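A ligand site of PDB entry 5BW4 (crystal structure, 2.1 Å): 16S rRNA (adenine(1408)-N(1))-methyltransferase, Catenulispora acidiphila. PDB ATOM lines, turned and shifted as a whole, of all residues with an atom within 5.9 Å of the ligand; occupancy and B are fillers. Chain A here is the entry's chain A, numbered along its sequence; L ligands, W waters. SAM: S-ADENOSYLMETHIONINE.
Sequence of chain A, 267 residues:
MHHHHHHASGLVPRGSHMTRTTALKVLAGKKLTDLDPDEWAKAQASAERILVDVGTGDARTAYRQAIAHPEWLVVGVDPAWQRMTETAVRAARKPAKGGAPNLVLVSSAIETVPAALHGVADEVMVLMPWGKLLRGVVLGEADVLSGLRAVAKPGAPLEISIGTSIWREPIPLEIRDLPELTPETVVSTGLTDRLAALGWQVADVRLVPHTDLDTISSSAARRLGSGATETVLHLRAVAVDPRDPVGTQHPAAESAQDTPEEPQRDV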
ATOM      1  N   ASP A  53      24.360  18.642   6.209  1.00  0.00           N
ATOM      2  CA  ASP A  53      23.279  19.292   6.966  1.00  0.00           C
ATOM      3  C   ASP A  53      22.799  18.352   8.123  1.00  0.00           C
ATOM      4  O   ASP A  53      22.154  17.270   7.947  1.00  0.00           O
ATOM      5  CB  ASP A  53      22.203  19.678   5.965  1.00  0.00           C
ATOM      6  CG  ASP A  53      21.092  20.569   6.534  1.00  0.00           C
ATOM      7  OD1 ASP A  53      21.422  21.553   7.249  1.00  0.00           O
ATOM      8  OD2 ASP A  53      19.886  20.308   6.221  1.00  0.00           O
ATOM      9  N   VAL A  54      23.160  18.700   9.338  1.00  0.00           N
ATOM     10  CA  VAL A  54      22.955  17.819  10.457  1.00  0.00           C
ATOM     11  C   VAL A  54      21.594  18.145  11.124  1.00  0.00           C
ATOM     12  O   VAL A  54      21.290  19.313  11.398  1.00  0.00           O
ATOM     13  CB  VAL A  54      24.130  17.909  11.449  1.00  0.00           C
ATOM     14  CG1 VAL A  54      23.920  16.996  12.657  1.00  0.00           C
ATOM     15  CG2 VAL A  54      25.431  17.518  10.780  1.00  0.00           C
ATOM     16  N   GLY A  55      20.778  17.127  11.356  1.00  0.00           N
ATOM     17  CA  GLY A  55      19.389  17.392  11.846  1.00  0.00           C
ATOM     18  C   GLY A  55      18.601  18.146  10.780  1.00  0.00           C
ATOM     19  O   GLY A  55      18.186  19.286  10.959  1.00  0.00           O
ATOM     20  N   THR A  56      18.351  17.482   9.680  1.00  0.00           N
ATOM     21  CA  THR A  56      17.793  18.140   8.468  1.00  0.00           C
ATOM     22  C   THR A  56      16.258  18.072   8.507  1.00  0.00           C
ATOM     23  O   THR A  56      15.579  18.796   7.798  1.00  0.00           O
ATOM     24  CB  THR A  56      18.415  17.499   7.203  1.00  0.00           C
ATOM     25  OG1 THR A  56      18.067  18.202   5.995  1.00  0.00           O
ATOM     26  CG2 THR A  56      17.983  16.062   7.102  1.00  0.00           C
ATOM     27  N   GLY A  57      15.716  17.220   9.375  1.00  0.00           N
ATOM     28  CA  GLY A  57      14.281  17.234   9.667  1.00  0.00           C
ATOM     29  C   GLY A  57      13.485  16.664   8.500  1.00  0.00           C
ATOM     30  O   GLY A  57      13.694  15.518   8.118  1.00  0.00           O
ATOM     31  N   ASP A  58      12.600  17.484   7.921  1.00  0.00           N
ATOM     32  CA  ASP A  58      11.853  17.045   6.722  1.00  0.00           C
ATOM     33  C   ASP A  58      12.672  17.194   5.454  1.00  0.00           C
ATOM     34  O   ASP A  58      12.266  16.716   4.449  1.00  0.00           O
ATOM     35  CB  ASP A  58      10.518  17.799   6.605  1.00  0.00           C
ATOM     36  CG  ASP A  58      10.701  19.286   6.287  1.00  0.00           C
ATOM     37  OD1 ASP A  58      11.807  19.769   5.936  1.00  0.00           O
ATOM     38  OD2 ASP A  58       9.689  19.990   6.389  1.00  0.00           O
ATOM     39  N   THR A  61      14.787  22.096   3.356  1.00  0.00           N
ATOM     40  CA  THR A  61      15.825  23.093   3.213  1.00  0.00           C
ATOM     41  C   THR A  61      17.029  22.457   2.458  1.00  0.00           C
ATOM     42  O   THR A  61      17.659  23.120   1.595  1.00  0.00           O
ATOM     43  CB  THR A  61      16.282  23.620   4.608  1.00  0.00           C
ATOM     44  OG1 THR A  61      15.179  24.218   5.272  1.00  0.00           O
ATOM     45  CG2 THR A  61      17.413  24.638   4.511  1.00  0.00           C
ATOM     46  N   VAL A  77      21.529  14.593   7.346  1.00  0.00           N
ATOM     47  CA  VAL A  77      21.731  13.525   8.320  1.00  0.00           C
ATOM     48  C   VAL A  77      20.667  13.746   9.384  1.00  0.00           C
ATOM     49  O   VAL A  77      20.528  14.865   9.949  1.00  0.00           O
ATOM     50  CB  VAL A  77      23.102  13.613   8.965  1.00  0.00           C
ATOM     51  CG1 VAL A  77      23.217  12.626  10.088  1.00  0.00           C
ATOM     52  CG2 VAL A  77      24.257  13.430   7.945  1.00  0.00           C
ATOM     53  N   ASP A  78      19.885  12.705   9.652  1.00  0.00           N
ATOM     54  CA  ASP A  78      18.914  12.744  10.727  1.00  0.00           C
ATOM     55  C   ASP A  78      18.593  11.312  11.159  1.00  0.00           C
ATOM     56  O   ASP A  78      18.348  10.442  10.324  1.00  0.00           O
ATOM     57  CB  ASP A  78      17.628  13.462  10.253  1.00  0.00           C
ATOM     58  CG  ASP A  78      16.776  14.027  11.447  1.00  0.00           C
ATOM     59  OD1 ASP A  78      16.369  13.229  12.312  1.00  0.00           O
ATOM     60  OD2 ASP A  78      16.548  15.260  11.479  1.00  0.00           O
ATOM     61  N   PRO A  79      18.592  11.042  12.459  1.00  0.00           N
ATOM     62  CA  PRO A  79      18.085   9.707  12.889  1.00  0.00           C
ATOM     63  C   PRO A  79      16.594   9.432  12.603  1.00  0.00           C
ATOM     64  O   PRO A  79      16.166   8.268  12.423  1.00  0.00           O
ATOM     65  CB  PRO A  79      18.303   9.709  14.412  1.00  0.00           C
ATOM     66  CG  PRO A  79      18.236  11.145  14.800  1.00  0.00           C
ATOM     67  CD  PRO A  79      18.815  11.939  13.592  1.00  0.00           C
ATOM     68  N   ALA A  80      15.785  10.477  12.579  1.00  0.00           N
ATOM     69  CA  ALA A  80      14.343  10.323  12.354  1.00  0.00           C
ATOM     70  C   ALA A  80      14.093  10.182  10.878  1.00  0.00           C
ATOM     71  O   ALA A  80      13.562  11.100  10.264  1.00  0.00           O
ATOM     72  CB  ALA A  80      13.624  11.559  12.880  1.00  0.00           C
ATOM     73  N   ARG A  83      10.689  10.991   8.672  1.00  0.00           N
ATOM     74  CA  ARG A  83      10.307  12.356   8.361  1.00  0.00           C
ATOM     75  C   ARG A  83      10.909  12.873   7.037  1.00  0.00           C
ATOM     76  O   ARG A  83      10.423  13.865   6.490  1.00  0.00           O
ATOM     77  CB  ARG A  83      10.767  13.265   9.486  1.00  0.00           C
ATOM     78  CG  ARG A  83       9.934  13.095  10.721  1.00  0.00           C
ATOM     79  CD  ARG A  83      10.637  13.720  11.905  1.00  0.00           C
ATOM     80  NE  ARG A  83      10.663  15.164  11.792  1.00  0.00           N
ATOM     81  CZ  ARG A  83      11.374  15.946  12.594  1.00  0.00           C
ATOM     82  NH1 ARG A  83      12.127  15.399  13.548  1.00  0.00           N
ATOM     83  NH2 ARG A  83      11.345  17.274  12.433  1.00  0.00           N
ATOM     84  N   SER A 108      21.120   8.551  10.476  1.00  0.00           N
ATOM     85  CA  SER A 108      22.097   8.390  11.554  1.00  0.00           C
ATOM     86  C   SER A 108      22.007   9.554  12.531  1.00  0.00           C
ATOM     87  O   SER A 108      21.525  10.623  12.224  1.00  0.00           O
ATOM     88  CB  SER A 108      23.497   8.310  10.980  1.00  0.00           C
ATOM     89  OG  SER A 108      24.428   8.477  11.999  1.00  0.00           O
ATOM     90  N   ALA A 109      22.449   9.299  13.746  1.00  0.00           N
ATOM     91  CA  ALA A 109      22.561  10.308  14.778  1.00  0.00           C
ATOM     92  C   ALA A 109      23.965  10.859  14.628  1.00  0.00           C
ATOM     93  O   ALA A 109      24.873  10.108  14.269  1.00  0.00           O
ATOM     94  CB  ALA A 109      22.350   9.648  16.131  1.00  0.00           C
ATOM     95  N   ILE A 110      24.175  12.140  14.922  1.00  0.00           N
ATOM     96  CA  ILE A 110      25.525  12.739  14.723  1.00  0.00           C
ATOM     97  C   ILE A 110      26.552  12.188  15.695  1.00  0.00           C
ATOM     98  O   ILE A 110      27.711  12.076  15.403  1.00  0.00           O
ATOM     99  CB  ILE A 110      25.506  14.297  14.808  1.00  0.00           C
ATOM    100  CG1 ILE A 110      26.819  14.907  14.289  1.00  0.00           C
ATOM    101  CG2 ILE A 110      25.253  14.729  16.227  1.00  0.00           C
ATOM    102  CD1 ILE A 110      27.155  14.540  12.856  1.00  0.00           C
ATOM    103  N   GLU A 111      26.124  11.821  16.880  1.00  0.00           N
ATOM    104  CA  GLU A 111      27.057  11.307  17.857  1.00  0.00           C
ATOM    105  C   GLU A 111      27.580   9.880  17.548  1.00  0.00           C
ATOM    106  O   GLU A 111      28.609   9.499  17.996  1.00  0.00           O
ATOM    107  CB  GLU A 111      26.465  11.427  19.297  1.00  0.00           C
ATOM    108  CG  GLU A 111      25.262  10.516  19.603  1.00  0.00           C
ATOM    109  CD  GLU A 111      23.888  11.111  19.278  1.00  0.00           C
ATOM    110  OE1 GLU A 111      23.780  12.072  18.478  1.00  0.00           O
ATOM    111  OE2 GLU A 111      22.894  10.572  19.832  1.00  0.00           O
ATOM    112  N   VAL A 126      24.178  23.234  11.162  1.00  0.00           N
ATOM    113  CA  VAL A 126      23.219  22.796  12.123  1.00  0.00           C
ATOM    114  C   VAL A 126      22.206  23.943  12.221  1.00  0.00           C
ATOM    115  O   VAL A 126      22.439  24.980  12.925  1.00  0.00           O
ATOM    116  CB  VAL A 126      23.880  22.553  13.475  1.00  0.00           C
ATOM    117  CG1 VAL A 126      22.831  22.098  14.468  1.00  0.00           C
ATOM    118  CG2 VAL A 126      24.964  21.490  13.383  1.00  0.00           C
ATOM    119  N   LEU A 127      21.141  23.830  11.480  1.00  0.00           N
ATOM    120  CA  LEU A 127      20.152  24.907  11.375  1.00  0.00           C
ATOM    121  C   LEU A 127      18.916  24.594  12.234  1.00  0.00           C
ATOM    122  O   LEU A 127      18.236  23.576  12.026  1.00  0.00           O
ATOM    123  CB  LEU A 127      19.714  25.063   9.906  1.00  0.00           C
ATOM    124  CG  LEU A 127      20.491  25.989   8.945  1.00  0.00           C
ATOM    125  CD1 LEU A 127      22.006  26.048   9.195  1.00  0.00           C
ATOM    126  CD2 LEU A 127      20.157  25.620   7.486  1.00  0.00           C
ATOM    127  N   MET A 128      18.570  25.495  13.169  1.00  0.00           N
ATOM    128  CA  MET A 128      17.423  25.295  14.072  1.00  0.00           C
ATOM    129  C   MET A 128      17.306  23.872  14.620  1.00  0.00           C
ATOM    130  O   MET A 128      16.271  23.234  14.503  1.00  0.00           O
ATOM    131  CB  MET A 128      16.098  25.635  13.341  1.00  0.00           C
ATOM    132  CG  MET A 128      16.175  26.902  12.500  1.00  0.00           C
ATOM    133  SD  MET A 128      16.462  28.317  13.615  1.00  0.00           S
ATOM    134  CE  MET A 128      16.683  29.634  12.405  1.00  0.00           C
ATOM    135  N   PRO A 129      18.346  23.378  15.321  1.00  0.00           N
ATOM    136  CA  PRO A 129      18.183  22.094  15.908  1.00  0.00           C
ATOM    137  C   PRO A 129      17.145  21.973  17.028  1.00  0.00           C
ATOM    138  O   PRO A 129      16.816  22.896  17.695  1.00  0.00           O
ATOM    139  CB  PRO A 129      19.577  21.820  16.519  1.00  0.00           C
ATOM    140  CG  PRO A 129      20.066  23.180  16.915  1.00  0.00           C
ATOM    141  CD  PRO A 129      19.539  24.089  15.845  1.00  0.00           C
ATOM    142  N   TRP A 130      16.720  20.752  17.276  1.00  0.00           N
ATOM    143  CA  TRP A 130      16.115  20.414  18.530  1.00  0.00           C
ATOM    144  C   TRP A 130      16.630  19.110  19.079  1.00  0.00           C
ATOM    145  O   TRP A 130      17.558  18.524  18.537  1.00  0.00           O
ATOM    146  CB  TRP A 130      14.600  20.506  18.507  1.00  0.00           C
ATOM    147  CG  TRP A 130      13.766  20.049  17.403  1.00  0.00           C
ATOM    148  CD1 TRP A 130      13.183  20.833  16.429  1.00  0.00           C
ATOM    149  CD2 TRP A 130      13.171  18.732  17.261  1.00  0.00           C
ATOM    150  NE1 TRP A 130      12.305  20.061  15.662  1.00  0.00           N
ATOM    151  CE2 TRP A 130      12.309  18.773  16.142  1.00  0.00           C
ATOM    152  CE3 TRP A 130      13.313  17.511  17.985  1.00  0.00           C
ATOM    153  CZ2 TRP A 130      11.600  17.635  15.692  1.00  0.00           C
ATOM    154  CZ3 TRP A 130      12.616  16.355  17.515  1.00  0.00           C
ATOM    155  CH2 TRP A 130      11.765  16.436  16.376  1.00  0.00           C
ATOM    156  N   GLY A 131      16.106  18.737  20.237  1.00  0.00           N
ATOM    157  CA  GLY A 131      16.437  17.507  20.910  1.00  0.00           C
ATOM    158  C   GLY A 131      17.889  17.465  21.333  1.00  0.00           C
ATOM    159  O   GLY A 131      18.484  18.468  21.715  1.00  0.00           O
ATOM    160  N   LYS A 132      18.458  16.289  21.222  1.00  0.00           N
ATOM    161  CA  LYS A 132      19.838  16.065  21.585  1.00  0.00           C
ATOM    162  C   LYS A 132      20.838  17.005  20.888  1.00  0.00           C
ATOM    163  O   LYS A 132      21.805  17.437  21.483  1.00  0.00           O
ATOM    164  CB  LYS A 132      20.138  14.649  21.280  1.00  0.00           C
ATOM    165  CG  LYS A 132      21.523  14.180  21.456  1.00  0.00           C
ATOM    166  CD  LYS A 132      22.005  14.269  22.816  1.00  0.00           C
ATOM    167  CE  LYS A 132      22.800  12.984  23.089  1.00  0.00           C
ATOM    168  NZ  LYS A 132      23.308  13.116  24.499  1.00  0.00           N
ATOM    169  N   LEU A 133      20.619  17.271  19.608  1.00  0.00           N
ATOM    170  CA  LEU A 133      21.481  18.136  18.824  1.00  0.00           C
ATOM    171  C   LEU A 133      21.514  19.558  19.377  1.00  0.00           C
ATOM    172  O   LEU A 133      22.612  20.120  19.553  1.00  0.00           O
ATOM    173  CB  LEU A 133      21.028  18.063  17.359  1.00  0.00           C
ATOM    174  CG  LEU A 133      21.897  18.852  16.326  1.00  0.00           C
ATOM    175  CD1 LEU A 133      23.352  18.378  16.259  1.00  0.00           C
ATOM    176  CD2 LEU A 133      21.286  18.742  14.943  1.00  0.00           C
ATOM    177  N   LEU A 134      20.328  20.085  19.763  1.00  0.00           N
ATOM    178  CA  LEU A 134      20.185  21.419  20.319  1.00  0.00           C
ATOM    179  C   LEU A 134      20.834  21.495  21.730  1.00  0.00           C
ATOM    180  O   LEU A 134      21.725  22.276  21.981  1.00  0.00           O
ATOM    181  CB  LEU A 134      18.666  21.841  20.404  1.00  0.00           C
ATOM    182  CG  LEU A 134      18.426  23.092  21.235  1.00  0.00           C
ATOM    183  CD1 LEU A 134      19.123  24.228  20.537  1.00  0.00           C
ATOM    184  CD2 LEU A 134      16.902  23.342  21.352  1.00  0.00           C
ATOM    185  N   VAL A 144      28.237  15.078  20.833  1.00  0.00           N
ATOM    186  CA  VAL A 144      27.696  15.882  19.725  1.00  0.00           C
ATOM    187  C   VAL A 144      28.780  16.710  18.982  1.00  0.00           C
ATOM    188  O   VAL A 144      28.868  16.603  17.786  1.00  0.00           O
ATOM    189  CB  VAL A 144      26.591  16.826  20.231  1.00  0.00           C
ATOM    190  CG1 VAL A 144      26.215  17.835  19.193  1.00  0.00           C
ATOM    191  CG2 VAL A 144      25.415  15.995  20.675  1.00  0.00           C
HETATM  192  N   SAM L   1      17.406  21.879  10.089  1.00  0.00           N
HETATM  193  CA  SAM L   1      16.044  21.906   9.474  1.00  0.00           C
HETATM  194  C   SAM L   1      15.554  23.321   9.196  1.00  0.00           C
HETATM  195  O   SAM L   1      15.977  23.912   8.174  1.00  0.00           O
HETATM  196  OXT SAM L   1      14.747  23.885   9.980  1.00  0.00           O
HETATM  197  CB  SAM L   1      15.006  21.153  10.333  1.00  0.00           C
HETATM  198  CG  SAM L   1      15.283  21.217  11.844  1.00  0.00           C
HETATM  199  SD  SAM L   1      14.498  19.981  12.682  1.00  0.00           S
HETATM  200  CE  SAM L   1      13.011  20.693  12.897  1.00  0.00           C
HETATM  201  C5' SAM L   1      15.385  19.487  14.032  1.00  0.00           C
HETATM  202  C4' SAM L   1      16.082  18.161  13.740  1.00  0.00           C
HETATM  203  O4' SAM L   1      17.250  17.887  14.534  1.00  0.00           O
HETATM  204  C3' SAM L   1      15.093  17.019  14.029  1.00  0.00           C
HETATM  205  O3' SAM L   1      14.643  16.330  12.879  1.00  0.00           O
HETATM  206  C2' SAM L   1      15.844  16.050  14.900  1.00  0.00           C
HETATM  207  O2' SAM L   1      15.602  14.694  14.581  1.00  0.00           O
HETATM  208  C1' SAM L   1      17.276  16.455  14.599  1.00  0.00           C
HETATM  209  N9  SAM L   1      18.126  15.795  15.599  1.00  0.00           N
HETATM  210  C8  SAM L   1      17.927  15.741  16.937  1.00  0.00           C
HETATM  211  N7  SAM L   1      18.908  15.087  17.561  1.00  0.00           N
HETATM  212  C5  SAM L   1      19.774  14.737  16.577  1.00  0.00           C
HETATM  213  C6  SAM L   1      21.010  14.018  16.557  1.00  0.00           C
HETATM  214  N6  SAM L   1      21.493  13.574  17.710  1.00  0.00           N
HETATM  215  N1  SAM L   1      21.640  13.870  15.388  1.00  0.00           N
HETATM  216  C2  SAM L   1      21.133  14.310  14.273  1.00  0.00           C
HETATM  217  N3  SAM L   1      19.996  15.006  14.187  1.00  0.00           N
HETATM  218  C4  SAM L   1      19.277  15.181  15.318  1.00  0.00           C
HETATM  219  O   HOH W   1      20.735  21.533   9.755  1.00  0.00           O
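O3' of the ligand is in hydrogen-bond range of OD2 of Asp 78 (2.6 Å). N of the ligand is in hydrogen-bond range of O of Leu 127 (2.7 Å). The guanidinium group (NH1) of Arg 83 sits at hydrogen-bond distance from an oxygen (O3') of the ligand (2.8 Å). The side-chain carboxylate (OE1) of Glu 111 sits at hydrogen-bond distance from a nitrogen (N6) of the ligand (2.8 Å). O of Gly 55 is in hydrogen-bond range of N of the ligand. The side-chain hydroxyl (OG1) of Thr 61 sits at hydrogen-bond distance from an oxygen (O) of the ligand (3.0 Å). The backbone NH (N) of Ile 110 lies within hydrogen-bond range of a nitrogen (N1) of the ligand, at 3.1 Å. The backbone NH (N) of Leu 133 sits at hydrogen-bond distance from a nitrogen (N7) of the ligand, at 3.4 Å.
The side-chain carboxylate (OD2) of Asp 78 sits at hydrogen-bond distance from the backbone NH (N) of Gly 57, 3.0 Å away. The side-chain carboxylate (OD2) of Asp 78 is in hydrogen-bond range of the backbone NH (N) of Thr 56, at 3.4 Å. The side-chain carboxylate (OD1) of Asp 78 is in hydrogen-bond range of the backbone NH (N) of Ala 80 (2.8 Å). The backbone carbonyl oxygen (O) of Asp 78 sits at hydrogen-bond distance from the backbone NH (N) of Ser 108 (3.4 Å). N of Gly 55 is in hydrogen-bond range of O of Val 77 (2.7 Å). The backbone carbonyl oxygen (O) of Val 77 sits at hydrogen-bond distance from the backbone NH (N) of Thr 56 (3.4 Å). The side-chain hydroxyl of Thr 56 is in hydrogen-bond range of the side-chain carboxylate of Asp 53.
NE1 of Trp 130 sits close to SD of the ligand, at 3.7 Å. Thr 56 touches the ligand (O to CB, 3.5 Å). Gly 57 touches the ligand. CD of Pro 79 touches N3 of the ligand (3.3 Å). Ala 109 touches the ligand. Met 128 touches the ligand (O to CG, 3.5 Å). CG of Lys 132 touches N6 of the ligand, at 3.8 Å. Hydrophobic or aromatic side chains within 4 Å of the ligand: Pro 79, Ile 110, Leu 127, Trp 130 and Leu 133. 15 residues have an atom within 4 Å of the ligand: Gly 55, Thr 56, Gly 57, Thr 61, Asp 78, Pro 79, Arg 83, Ala 109, Ile 110, Glu 111, Leu 127, Met 128, Trp 130, Lys 132 and Leu 133.
Water W1 lies within hydrogen-bond range of OD1 of Asp 53 (2.6 Å), O of Val 54 (2.8 Å), N of Leu 127 (2.9 Å) and N of the ligand (3.4 Å).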
